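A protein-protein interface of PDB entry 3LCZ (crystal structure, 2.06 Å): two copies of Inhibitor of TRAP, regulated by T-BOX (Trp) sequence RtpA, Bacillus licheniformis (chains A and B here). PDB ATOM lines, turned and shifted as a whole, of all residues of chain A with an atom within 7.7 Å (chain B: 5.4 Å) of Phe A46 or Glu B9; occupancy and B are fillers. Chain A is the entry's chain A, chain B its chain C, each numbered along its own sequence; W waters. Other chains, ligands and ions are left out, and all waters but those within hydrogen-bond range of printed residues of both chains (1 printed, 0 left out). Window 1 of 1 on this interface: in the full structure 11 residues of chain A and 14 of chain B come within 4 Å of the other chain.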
ATOM      1  N   GLY A  40     -10.592  31.985 -25.875  1.00  0.00           N
ATOM      2  CA  GLY A  40     -11.290  32.343 -24.631  1.00  0.00           C
ATOM      3  C   GLY A  40     -12.795  32.317 -24.808  1.00  0.00           C
ATOM      4  O   GLY A  40     -13.480  31.743 -23.978  1.00  0.00           O
ATOM      5  N   SER A  41     -13.314  32.944 -25.868  1.00  0.00           N
ATOM      6  CA  SER A  41     -14.772  32.904 -26.184  1.00  0.00           C
ATOM      7  C   SER A  41     -15.279  31.489 -26.391  1.00  0.00           C
ATOM      8  O   SER A  41     -16.352  31.112 -25.929  1.00  0.00           O
ATOM      9  CB  SER A  41     -15.096  33.653 -27.480  1.00  0.00           C
ATOM     10  OG  SER A  41     -14.596  34.959 -27.459  1.00  0.00           O
ATOM     11  N   THR A  42     -14.536  30.734 -27.177  1.00  0.00           N
ATOM     12  CA  THR A  42     -14.848  29.340 -27.390  1.00  0.00           C
ATOM     13  C   THR A  42     -15.018  28.587 -26.059  1.00  0.00           C
ATOM     14  O   THR A  42     -16.009  27.880 -25.838  1.00  0.00           O
ATOM     15  CB  THR A  42     -13.744  28.703 -28.211  1.00  0.00           C
ATOM     16  OG1 THR A  42     -13.780  29.287 -29.502  1.00  0.00           O
ATOM     17  CG2 THR A  42     -13.964  27.179 -28.358  1.00  0.00           C
ATOM     18  N   LEU A  43     -14.066  28.760 -25.155  1.00  0.00           N
ATOM     19  CA  LEU A  43     -14.153  28.083 -23.856  1.00  0.00           C
ATOM     20  C   LEU A  43     -15.282  28.581 -22.962  1.00  0.00           C
ATOM     21  O   LEU A  43     -15.971  27.773 -22.338  1.00  0.00           O
ATOM     22  CB  LEU A  43     -12.835  28.189 -23.101  1.00  0.00           C
ATOM     23  CG  LEU A  43     -11.684  27.640 -23.936  1.00  0.00           C
ATOM     24  CD1 LEU A  43     -10.394  27.571 -23.123  1.00  0.00           C
ATOM     25  CD2 LEU A  43     -12.069  26.274 -24.424  1.00  0.00           C
ATOM     26  N   LEU A  44     -15.432  29.902 -22.866  1.00  0.00           N
ATOM     27  CA  LEU A  44     -16.417  30.492 -22.003  1.00  0.00           C
ATOM     28  C   LEU A  44     -17.761  30.019 -22.548  1.00  0.00           C
ATOM     29  O   LEU A  44     -18.593  29.474 -21.827  1.00  0.00           O
ATOM     30  CB  LEU A  44     -16.334  32.045 -22.021  1.00  0.00           C
ATOM     31  CG  LEU A  44     -17.318  32.708 -21.042  1.00  0.00           C
ATOM     32  CD1 LEU A  44     -16.964  32.337 -19.635  1.00  0.00           C
ATOM     33  CD2 LEU A  44     -17.392  34.220 -21.167  1.00  0.00           C
ATOM     34  N   HIS A  45     -17.956  30.219 -23.840  1.00  0.00           N
ATOM     35  CA  HIS A  45     -19.187  29.808 -24.483  1.00  0.00           C
ATOM     36  C   HIS A  45     -19.576  28.355 -24.182  1.00  0.00           C
ATOM     37  O   HIS A  45     -20.699  28.092 -23.828  1.00  0.00           O
ATOM     38  CB  HIS A  45     -19.104  30.093 -25.979  1.00  0.00           C
ATOM     39  CG  HIS A  45     -19.207  31.550 -26.321  1.00  0.00           C
ATOM     40  ND1 HIS A  45     -19.885  32.008 -27.433  1.00  0.00           N
ATOM     41  CD2 HIS A  45     -18.776  32.655 -25.663  1.00  0.00           C
ATOM     42  CE1 HIS A  45     -19.829  33.327 -27.468  1.00  0.00           C
ATOM     43  NE2 HIS A  45     -19.155  33.744 -26.410  1.00  0.00           N
ATOM     44  N   PHE A  46     -18.656  27.415 -24.351  1.00  0.00           N
ATOM     45  CA  PHE A  46     -18.921  25.996 -24.053  1.00  0.00           C
ATOM     46  C   PHE A  46     -19.322  25.708 -22.600  1.00  0.00           C
ATOM     47  O   PHE A  46     -20.256  24.950 -22.343  1.00  0.00           O
ATOM     48  CB  PHE A  46     -17.707  25.156 -24.397  1.00  0.00           C
ATOM     49  CG  PHE A  46     -17.794  23.724 -23.908  1.00  0.00           C
ATOM     50  CD1 PHE A  46     -17.144  23.327 -22.735  1.00  0.00           C
ATOM     51  CD2 PHE A  46     -18.501  22.780 -24.632  1.00  0.00           C
ATOM     52  CE1 PHE A  46     -17.187  22.005 -22.307  1.00  0.00           C
ATOM     53  CE2 PHE A  46     -18.605  21.466 -24.176  1.00  0.00           C
ATOM     54  CZ  PHE A  46     -17.929  21.078 -23.020  1.00  0.00           C
ATOM     55  N   ILE A  47     -18.583  26.272 -21.648  1.00  0.00           N
ATOM     56  CA  ILE A  47     -18.904  26.095 -20.241  1.00  0.00           C
ATOM     57  C   ILE A  47     -20.294  26.654 -19.933  1.00  0.00           C
ATOM     58  O   ILE A  47     -21.105  26.020 -19.222  1.00  0.00           O
ATOM     59  CB  ILE A  47     -17.868  26.827 -19.328  1.00  0.00           C
ATOM     60  CG1 ILE A  47     -16.487  26.220 -19.488  1.00  0.00           C
ATOM     61  CG2 ILE A  47     -18.302  26.775 -17.854  1.00  0.00           C
ATOM     62  CD1 ILE A  47     -16.436  24.741 -19.255  1.00  0.00           C
ATOM     63  N   LYS A  48     -20.564  27.851 -20.451  1.00  0.00           N
ATOM     64  CA  LYS A  48     -21.845  28.492 -20.192  1.00  0.00           C
ATOM     65  C   LYS A  48     -23.005  27.690 -20.754  1.00  0.00           C
ATOM     66  O   LYS A  48     -24.060  27.610 -20.153  1.00  0.00           O
ATOM     67  CB  LYS A  48     -21.858  29.905 -20.782  1.00  0.00           C
ATOM     68  CG  LYS A  48     -21.229  30.942 -19.864  1.00  0.00           C
ATOM     69  CD  LYS A  48     -20.874  32.230 -20.611  1.00  0.00           C
ATOM     70  CE  LYS A  48     -22.067  33.095 -20.966  1.00  0.00           C
ATOM     71  NZ  LYS A  48     -22.445  34.027 -19.854  1.00  0.00           N
ATOM     72  N   LYS A  49     -22.789  27.078 -21.906  1.00  0.00           N
ATOM     73  CA  LYS A  49     -23.826  26.362 -22.606  1.00  0.00           C
ATOM     74  C   LYS A  49     -24.220  25.102 -21.902  1.00  0.00           C
ATOM     75  O   LYS A  49     -25.339  24.622 -22.066  1.00  0.00           O
ATOM     76  CB  LYS A  49     -23.307  26.008 -23.998  1.00  0.00           C
ATOM     77  CG  LYS A  49     -24.275  25.273 -24.875  1.00  0.00           C
ATOM     78  CD  LYS A  49     -23.755  25.285 -26.304  1.00  0.00           C
ATOM     79  CE  LYS A  49     -24.632  24.503 -27.236  1.00  0.00           C
ATOM     80  NZ  LYS A  49     -24.074  24.596 -28.607  1.00  0.00           N
ATOM     81  N   HIS A  50     -23.278  24.540 -21.156  1.00  0.00           N
ATOM     82  CA  HIS A  50     -23.466  23.259 -20.500  1.00  0.00           C
ATOM     83  C   HIS A  50     -23.298  23.341 -18.985  1.00  0.00           C
ATOM     84  O   HIS A  50     -23.198  22.327 -18.323  1.00  0.00           O
ATOM     85  CB  HIS A  50     -22.448  22.257 -21.060  1.00  0.00           C
ATOM     86  CG  HIS A  50     -22.515  22.080 -22.546  1.00  0.00           C
ATOM     87  ND1 HIS A  50     -23.480  21.310 -23.161  1.00  0.00           N
ATOM     88  CD2 HIS A  50     -21.720  22.544 -23.535  1.00  0.00           C
ATOM     89  CE1 HIS A  50     -23.285  21.322 -24.466  1.00  0.00           C
ATOM     90  NE2 HIS A  50     -22.214  22.054 -24.717  1.00  0.00           N
ATOM     91  N   ILE A  51     -23.244  24.554 -18.451  1.00  0.00           N
ATOM     92  CA  ILE A  51     -23.030  24.799 -17.008  1.00  0.00           C
ATOM     93  C   ILE A  51     -23.994  24.003 -16.099  1.00  0.00           C
ATOM     94  O   ILE A  51     -23.608  23.462 -15.056  1.00  0.00           O
ATOM     95  CB  ILE A  51     -23.135  26.325 -16.707  1.00  0.00           C
ATOM     96  CG1 ILE A  51     -22.698  26.658 -15.280  1.00  0.00           C
ATOM     97  CG2 ILE A  51     -24.550  26.824 -16.963  1.00  0.00           C
ATOM     98  CD1 ILE A  51     -21.228  26.552 -15.052  1.00  0.00           C
ATOM     99  N   GLU A  53     -25.141  21.166 -16.431  1.00  0.00           N
ATOM    100  CA  GLU A  53     -25.079  19.736 -16.693  1.00  0.00           C
ATOM    101  C   GLU A  53     -23.711  19.132 -16.420  1.00  0.00           C
ATOM    102  O   GLU A  53     -23.552  17.918 -16.560  1.00  0.00           O
ATOM    103  CB  GLU A  53     -25.519  19.429 -18.115  1.00  0.00           C
ATOM    104  CG  GLU A  53     -24.510  19.808 -19.158  1.00  0.00           C
ATOM    105  CD  GLU A  53     -25.028  19.580 -20.563  1.00  0.00           C
ATOM    106  OE1 GLU A  53     -26.132  20.080 -20.879  1.00  0.00           O
ATOM    107  OE2 GLU A  53     -24.316  18.917 -21.350  1.00  0.00           O
ATOM    108  OXT GLU A  53     -22.762  19.826 -16.046  1.00  0.00           O
ATOM    109  N   THR B   5     -14.602  24.594 -30.746  1.00  0.00           N
ATOM    110  CA  THR B   5     -15.917  24.198 -30.295  1.00  0.00           C
ATOM    111  C   THR B   5     -16.233  22.761 -30.639  1.00  0.00           C
ATOM    112  O   THR B   5     -16.853  22.040 -29.856  1.00  0.00           O
ATOM    113  CB  THR B   5     -16.960  25.089 -30.942  1.00  0.00           C
ATOM    114  OG1 THR B   5     -16.940  26.363 -30.290  1.00  0.00           O
ATOM    115  CG2 THR B   5     -18.337  24.485 -30.793  1.00  0.00           C
ATOM    116  N   ASP B   6     -15.790  22.343 -31.816  1.00  0.00           N
ATOM    117  CA  ASP B   6     -16.119  21.028 -32.315  1.00  0.00           C
ATOM    118  C   ASP B   6     -15.288  19.915 -31.662  1.00  0.00           C
ATOM    119  O   ASP B   6     -15.583  18.727 -31.809  1.00  0.00           O
ATOM    120  CB  ASP B   6     -16.169  21.035 -33.860  1.00  0.00           C
ATOM    121  CG  ASP B   6     -14.801  21.226 -34.511  1.00  0.00           C
ATOM    122  OD1 ASP B   6     -13.765  21.167 -33.811  1.00  0.00           O
ATOM    123  OD2 ASP B   6     -14.758  21.410 -35.751  1.00  0.00           O
ATOM    124  N   ASP B   7     -14.309  20.337 -30.861  1.00  0.00           N
ATOM    125  CA  ASP B   7     -13.446  19.458 -30.066  1.00  0.00           C
ATOM    126  C   ASP B   7     -13.977  19.347 -28.676  1.00  0.00           C
ATOM    127  O   ASP B   7     -13.452  18.588 -27.872  1.00  0.00           O
ATOM    128  CB  ASP B   7     -12.074  20.098 -29.920  1.00  0.00           C
ATOM    129  CG  ASP B   7     -11.390  20.296 -31.247  1.00  0.00           C
ATOM    130  OD1 ASP B   7     -11.692  19.502 -32.171  1.00  0.00           O
ATOM    131  OD2 ASP B   7     -10.547  21.221 -31.344  1.00  0.00           O
ATOM    132  N   LEU B   8     -14.965  20.170 -28.360  1.00  0.00           N
ATOM    133  CA  LEU B   8     -15.571  20.142 -27.030  1.00  0.00           C
ATOM    134  C   LEU B   8     -16.942  19.488 -27.144  1.00  0.00           C
ATOM    135  O   LEU B   8     -17.437  18.863 -26.215  1.00  0.00           O
ATOM    136  CB  LEU B   8     -15.709  21.570 -26.506  1.00  0.00           C
ATOM    137  CG  LEU B   8     -14.448  22.329 -26.112  1.00  0.00           C
ATOM    138  CD1 LEU B   8     -14.717  23.830 -26.008  1.00  0.00           C
ATOM    139  CD2 LEU B   8     -13.915  21.778 -24.819  1.00  0.00           C
ATOM    140  N   GLU B   9     -17.574  19.624 -28.303  1.00  0.00           N
ATOM    141  CA  GLU B   9     -18.882  19.015 -28.447  1.00  0.00           C
ATOM    142  C   GLU B   9     -19.114  18.556 -29.865  1.00  0.00           C
ATOM    143  O   GLU B   9     -18.742  19.242 -30.815  1.00  0.00           O
ATOM    144  CB  GLU B   9     -19.957  20.008 -28.032  1.00  0.00           C
ATOM    145  CG  GLU B   9     -19.999  21.226 -28.909  1.00  0.00           C
ATOM    146  CD  GLU B   9     -20.890  22.287 -28.336  1.00  0.00           C
ATOM    147  OE1 GLU B   9     -21.029  22.311 -27.097  1.00  0.00           O
ATOM    148  OE2 GLU B   9     -21.434  23.102 -29.110  1.00  0.00           O
ATOM    149  N   THR B  10     -19.673  17.371 -30.027  1.00  0.00           N
ATOM    150  CA  THR B  10     -19.980  16.930 -31.367  1.00  0.00           C
ATOM    151  C   THR B  10     -21.476  16.744 -31.588  1.00  0.00           C
ATOM    152  O   THR B  10     -22.179  16.203 -30.724  1.00  0.00           O
ATOM    153  CB  THR B  10     -19.009  15.825 -31.944  1.00  0.00           C
ATOM    154  OG1 THR B  10     -18.462  15.021 -30.881  1.00  0.00           O
ATOM    155  CG2 THR B  10     -17.814  16.498 -32.666  1.00  0.00           C
ATOM    156  N   THR B  11     -21.966  17.272 -32.712  1.00  0.00           N
ATOM    157  CA  THR B  11     -23.391  17.204 -33.063  1.00  0.00           C
ATOM    158  C   THR B  11     -24.052  15.901 -32.616  1.00  0.00           C
ATOM    159  O   THR B  11     -23.486  14.823 -32.752  1.00  0.00           O
ATOM    160  CB  THR B  11     -23.652  17.482 -34.561  1.00  0.00           C
ATOM    161  OG1 THR B  11     -22.744  16.713 -35.353  1.00  0.00           O
ATOM    162  CG2 THR B  11     -23.432  18.953 -34.879  1.00  0.00           C
ATOM    163  N   VAL B  34     -26.281  19.091 -29.239  1.00  0.00           N
ATOM    164  CA  VAL B  34     -24.866  18.749 -29.324  1.00  0.00           C
ATOM    165  C   VAL B  34     -24.539  17.912 -28.105  1.00  0.00           C
ATOM    166  O   VAL B  34     -25.083  18.150 -27.039  1.00  0.00           O
ATOM    167  CB  VAL B  34     -23.972  20.002 -29.234  1.00  0.00           C
ATOM    168  CG1 VAL B  34     -24.284  20.986 -30.340  1.00  0.00           C
ATOM    169  CG2 VAL B  34     -24.131  20.654 -27.876  1.00  0.00           C
ATOM    170  N   ILE B  35     -23.672  16.916 -28.244  1.00  0.00           N
ATOM    171  CA  ILE B  35     -23.218  16.197 -27.053  1.00  0.00           C
ATOM    172  C   ILE B  35     -21.747  16.470 -26.780  1.00  0.00           C
ATOM    173  O   ILE B  35     -21.009  16.894 -27.671  1.00  0.00           O
ATOM    174  CB  ILE B  35     -23.442  14.690 -27.110  1.00  0.00           C
ATOM    175  CG1 ILE B  35     -22.632  14.068 -28.251  1.00  0.00           C
ATOM    176  CG2 ILE B  35     -24.918  14.383 -27.151  1.00  0.00           C
ATOM    177  CD1 ILE B  35     -22.292  12.611 -28.034  1.00  0.00           C
ATOM    178  N   LEU B  36     -21.328  16.188 -25.551  1.00  0.00           N
ATOM    179  CA  LEU B  36     -19.965  16.429 -25.099  1.00  0.00           C
ATOM    180  C   LEU B  36     -18.953  15.388 -25.548  1.00  0.00           C
ATOM    181  O   LEU B  36     -19.271  14.206 -25.650  1.00  0.00           O
ATOM    182  CB  LEU B  36     -19.930  16.498 -23.576  1.00  0.00           C
ATOM    183  CG  LEU B  36     -20.808  17.546 -22.894  1.00  0.00           C
ATOM    184  CD1 LEU B  36     -20.533  17.589 -21.378  1.00  0.00           C
ATOM    185  CD2 LEU B  36     -20.623  18.908 -23.542  1.00  0.00           C
ATOM    186  N   THR B  37     -17.718  15.845 -25.792  1.00  0.00           N
ATOM    187  CA  THR B  37     -16.602  14.962 -26.117  1.00  0.00           C
ATOM    188  C   THR B  37     -15.832  14.659 -24.834  1.00  0.00           C
ATOM    189  O   THR B  37     -16.125  15.201 -23.774  1.00  0.00           O
ATOM    190  CB  THR B  37     -15.608  15.596 -27.150  1.00  0.00           C
ATOM    191  OG1 THR B  37     -14.998  16.756 -26.583  1.00  0.00           O
ATOM    192  CG2 THR B  37     -16.290  15.959 -28.449  1.00  0.00           C
ATOM    193  N   GLY B  40     -14.459  17.913 -23.937  1.00  0.00           N
ATOM    194  CA  GLY B  40     -15.500  18.804 -23.454  1.00  0.00           C
ATOM    195  C   GLY B  40     -16.012  18.343 -22.100  1.00  0.00           C
ATOM    196  O   GLY B  40     -16.129  19.138 -21.170  1.00  0.00           O
ATOM    197  N   SER B  41     -16.355  17.060 -22.000  1.00  0.00           N
ATOM    198  CA  SER B  41     -16.755  16.477 -20.716  1.00  0.00           C
ATOM    199  C   SER B  41     -15.670  16.659 -19.633  1.00  0.00           C
ATOM    200  O   SER B  41     -15.967  16.969 -18.468  1.00  0.00           O
ATOM    201  CB  SER B  41     -17.136  14.995 -20.918  1.00  0.00           C
ATOM    202  OG  SER B  41     -16.939  14.255 -19.739  1.00  0.00           O
ATOM    203  N   LEU B  43     -13.376  19.101 -19.434  1.00  0.00           N
ATOM    204  CA  LEU B  43     -13.321  20.480 -18.977  1.00  0.00           C
ATOM    205  C   LEU B  43     -14.467  20.860 -18.088  1.00  0.00           C
ATOM    206  O   LEU B  43     -14.269  21.615 -17.139  1.00  0.00           O
ATOM    207  CB  LEU B  43     -13.286  21.484 -20.134  1.00  0.00           C
ATOM    208  CG  LEU B  43     -12.028  21.397 -20.998  1.00  0.00           C
ATOM    209  CD1 LEU B  43     -11.958  22.602 -22.000  1.00  0.00           C
ATOM    210  CD2 LEU B  43     -10.847  21.405 -20.066  1.00  0.00           C
ATOM    211  N   LEU B  44     -15.676  20.474 -18.506  1.00  0.00           N
ATOM    212  CA  LEU B  44     -16.900  20.769 -17.775  1.00  0.00           C
ATOM    213  C   LEU B  44     -16.893  20.141 -16.373  1.00  0.00           C
ATOM    214  O   LEU B  44     -17.316  20.765 -15.424  1.00  0.00           O
ATOM    215  CB  LEU B  44     -18.099  20.238 -18.544  1.00  0.00           C
ATOM    216  CG  LEU B  44     -19.495  20.557 -17.997  1.00  0.00           C
ATOM    217  CD1 LEU B  44     -19.884  21.986 -18.414  1.00  0.00           C
ATOM    218  CD2 LEU B  44     -20.464  19.553 -18.588  1.00  0.00           C
HETATM  219  O   HOH W   1     -17.534  27.044 -27.842  1.00  0.00           O
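Among the printed residues, pairs that only touch across the chains: Phe A46 with Gly B40, Phe A46 with Leu B36, His A50 with Leu B44, Glu A53 with Leu B44, Phe A46 with Leu B8, Phe A46 with Glu B9, His A50 with Val B34, Thr A42 with Thr B5, His A50 with Leu B36, Lys A49 with Val B34 and Leu A43 with Leu B8.
A ring nitrogen (ND1) of His A50 is in hydrogen-bond range of the side-chain carboxylate of Glu A53 (3.1 Å).
O of Leu B8 lies within hydrogen-bond range of N of Thr B37.
The backbone NH (N) of Gly B40 is in hydrogen-bond range of the side-chain hydroxyl (OG1) of Thr B37.
The side-chain amino group (NZ) of Lys A49 is in salt-bridge range of the side-chain carboxylate (OE2) of Glu B9, at 3.1 Å.
NE2 of His A50 lies within hydrogen-bond range of OE1 of Glu B9.
Of the 13 printed residues of chain A, 6 touch a printed residue of chain B.
Printed residues of chain A that touch a printed residue of chain B: Thr A42, Leu A43, Phe A46, Lys A49, His A50 and Glu A53.
Hydrophobic or aromatic side chains of chain A that line the printed part of chain B: Leu A43, Phe A46 and His A50.
Hydrophobic or aromatic side chains of chain B that line the printed part of chain A: Leu B8, Val B34, Leu B36 and Leu B44.
Along chain B the printed residues that touch a printed residue of chain A span positions 5 to 44.
Among the printed residues, Asp or Glu carboxylates within 4 Å of a Lys or Arg side-chain nitrogen of the other chain: Lys A49 with Glu B9 (3.1 Å).
4 positions are printed for both chains.
Of the 13 pairs that touch across the chains among the printed residues, none has its exchanged pair printed and touching as well.
Of chain B, only Leu B8, Glu B9, Leu B36 and Gly B40 come within 4 Å of Phe A46.
Glu B9 touches just these residues of chain A: Phe A46, Lys A49 and His A50.
Of the printed residues of chain A, Gly B40 touches Phe A46.
Of the printed residues of chain B, Leu A43 touches Leu B8.
Ile B35 touches none of the printed residues of chain A.
The nearest residue of chain A that does not touch Glu B9 is His A45 (6.6 Å).
Water W1 lies within hydrogen-bond range of the side-chain hydroxyl of Thr B5 and the backbone carbonyl oxygen of Thr A42.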
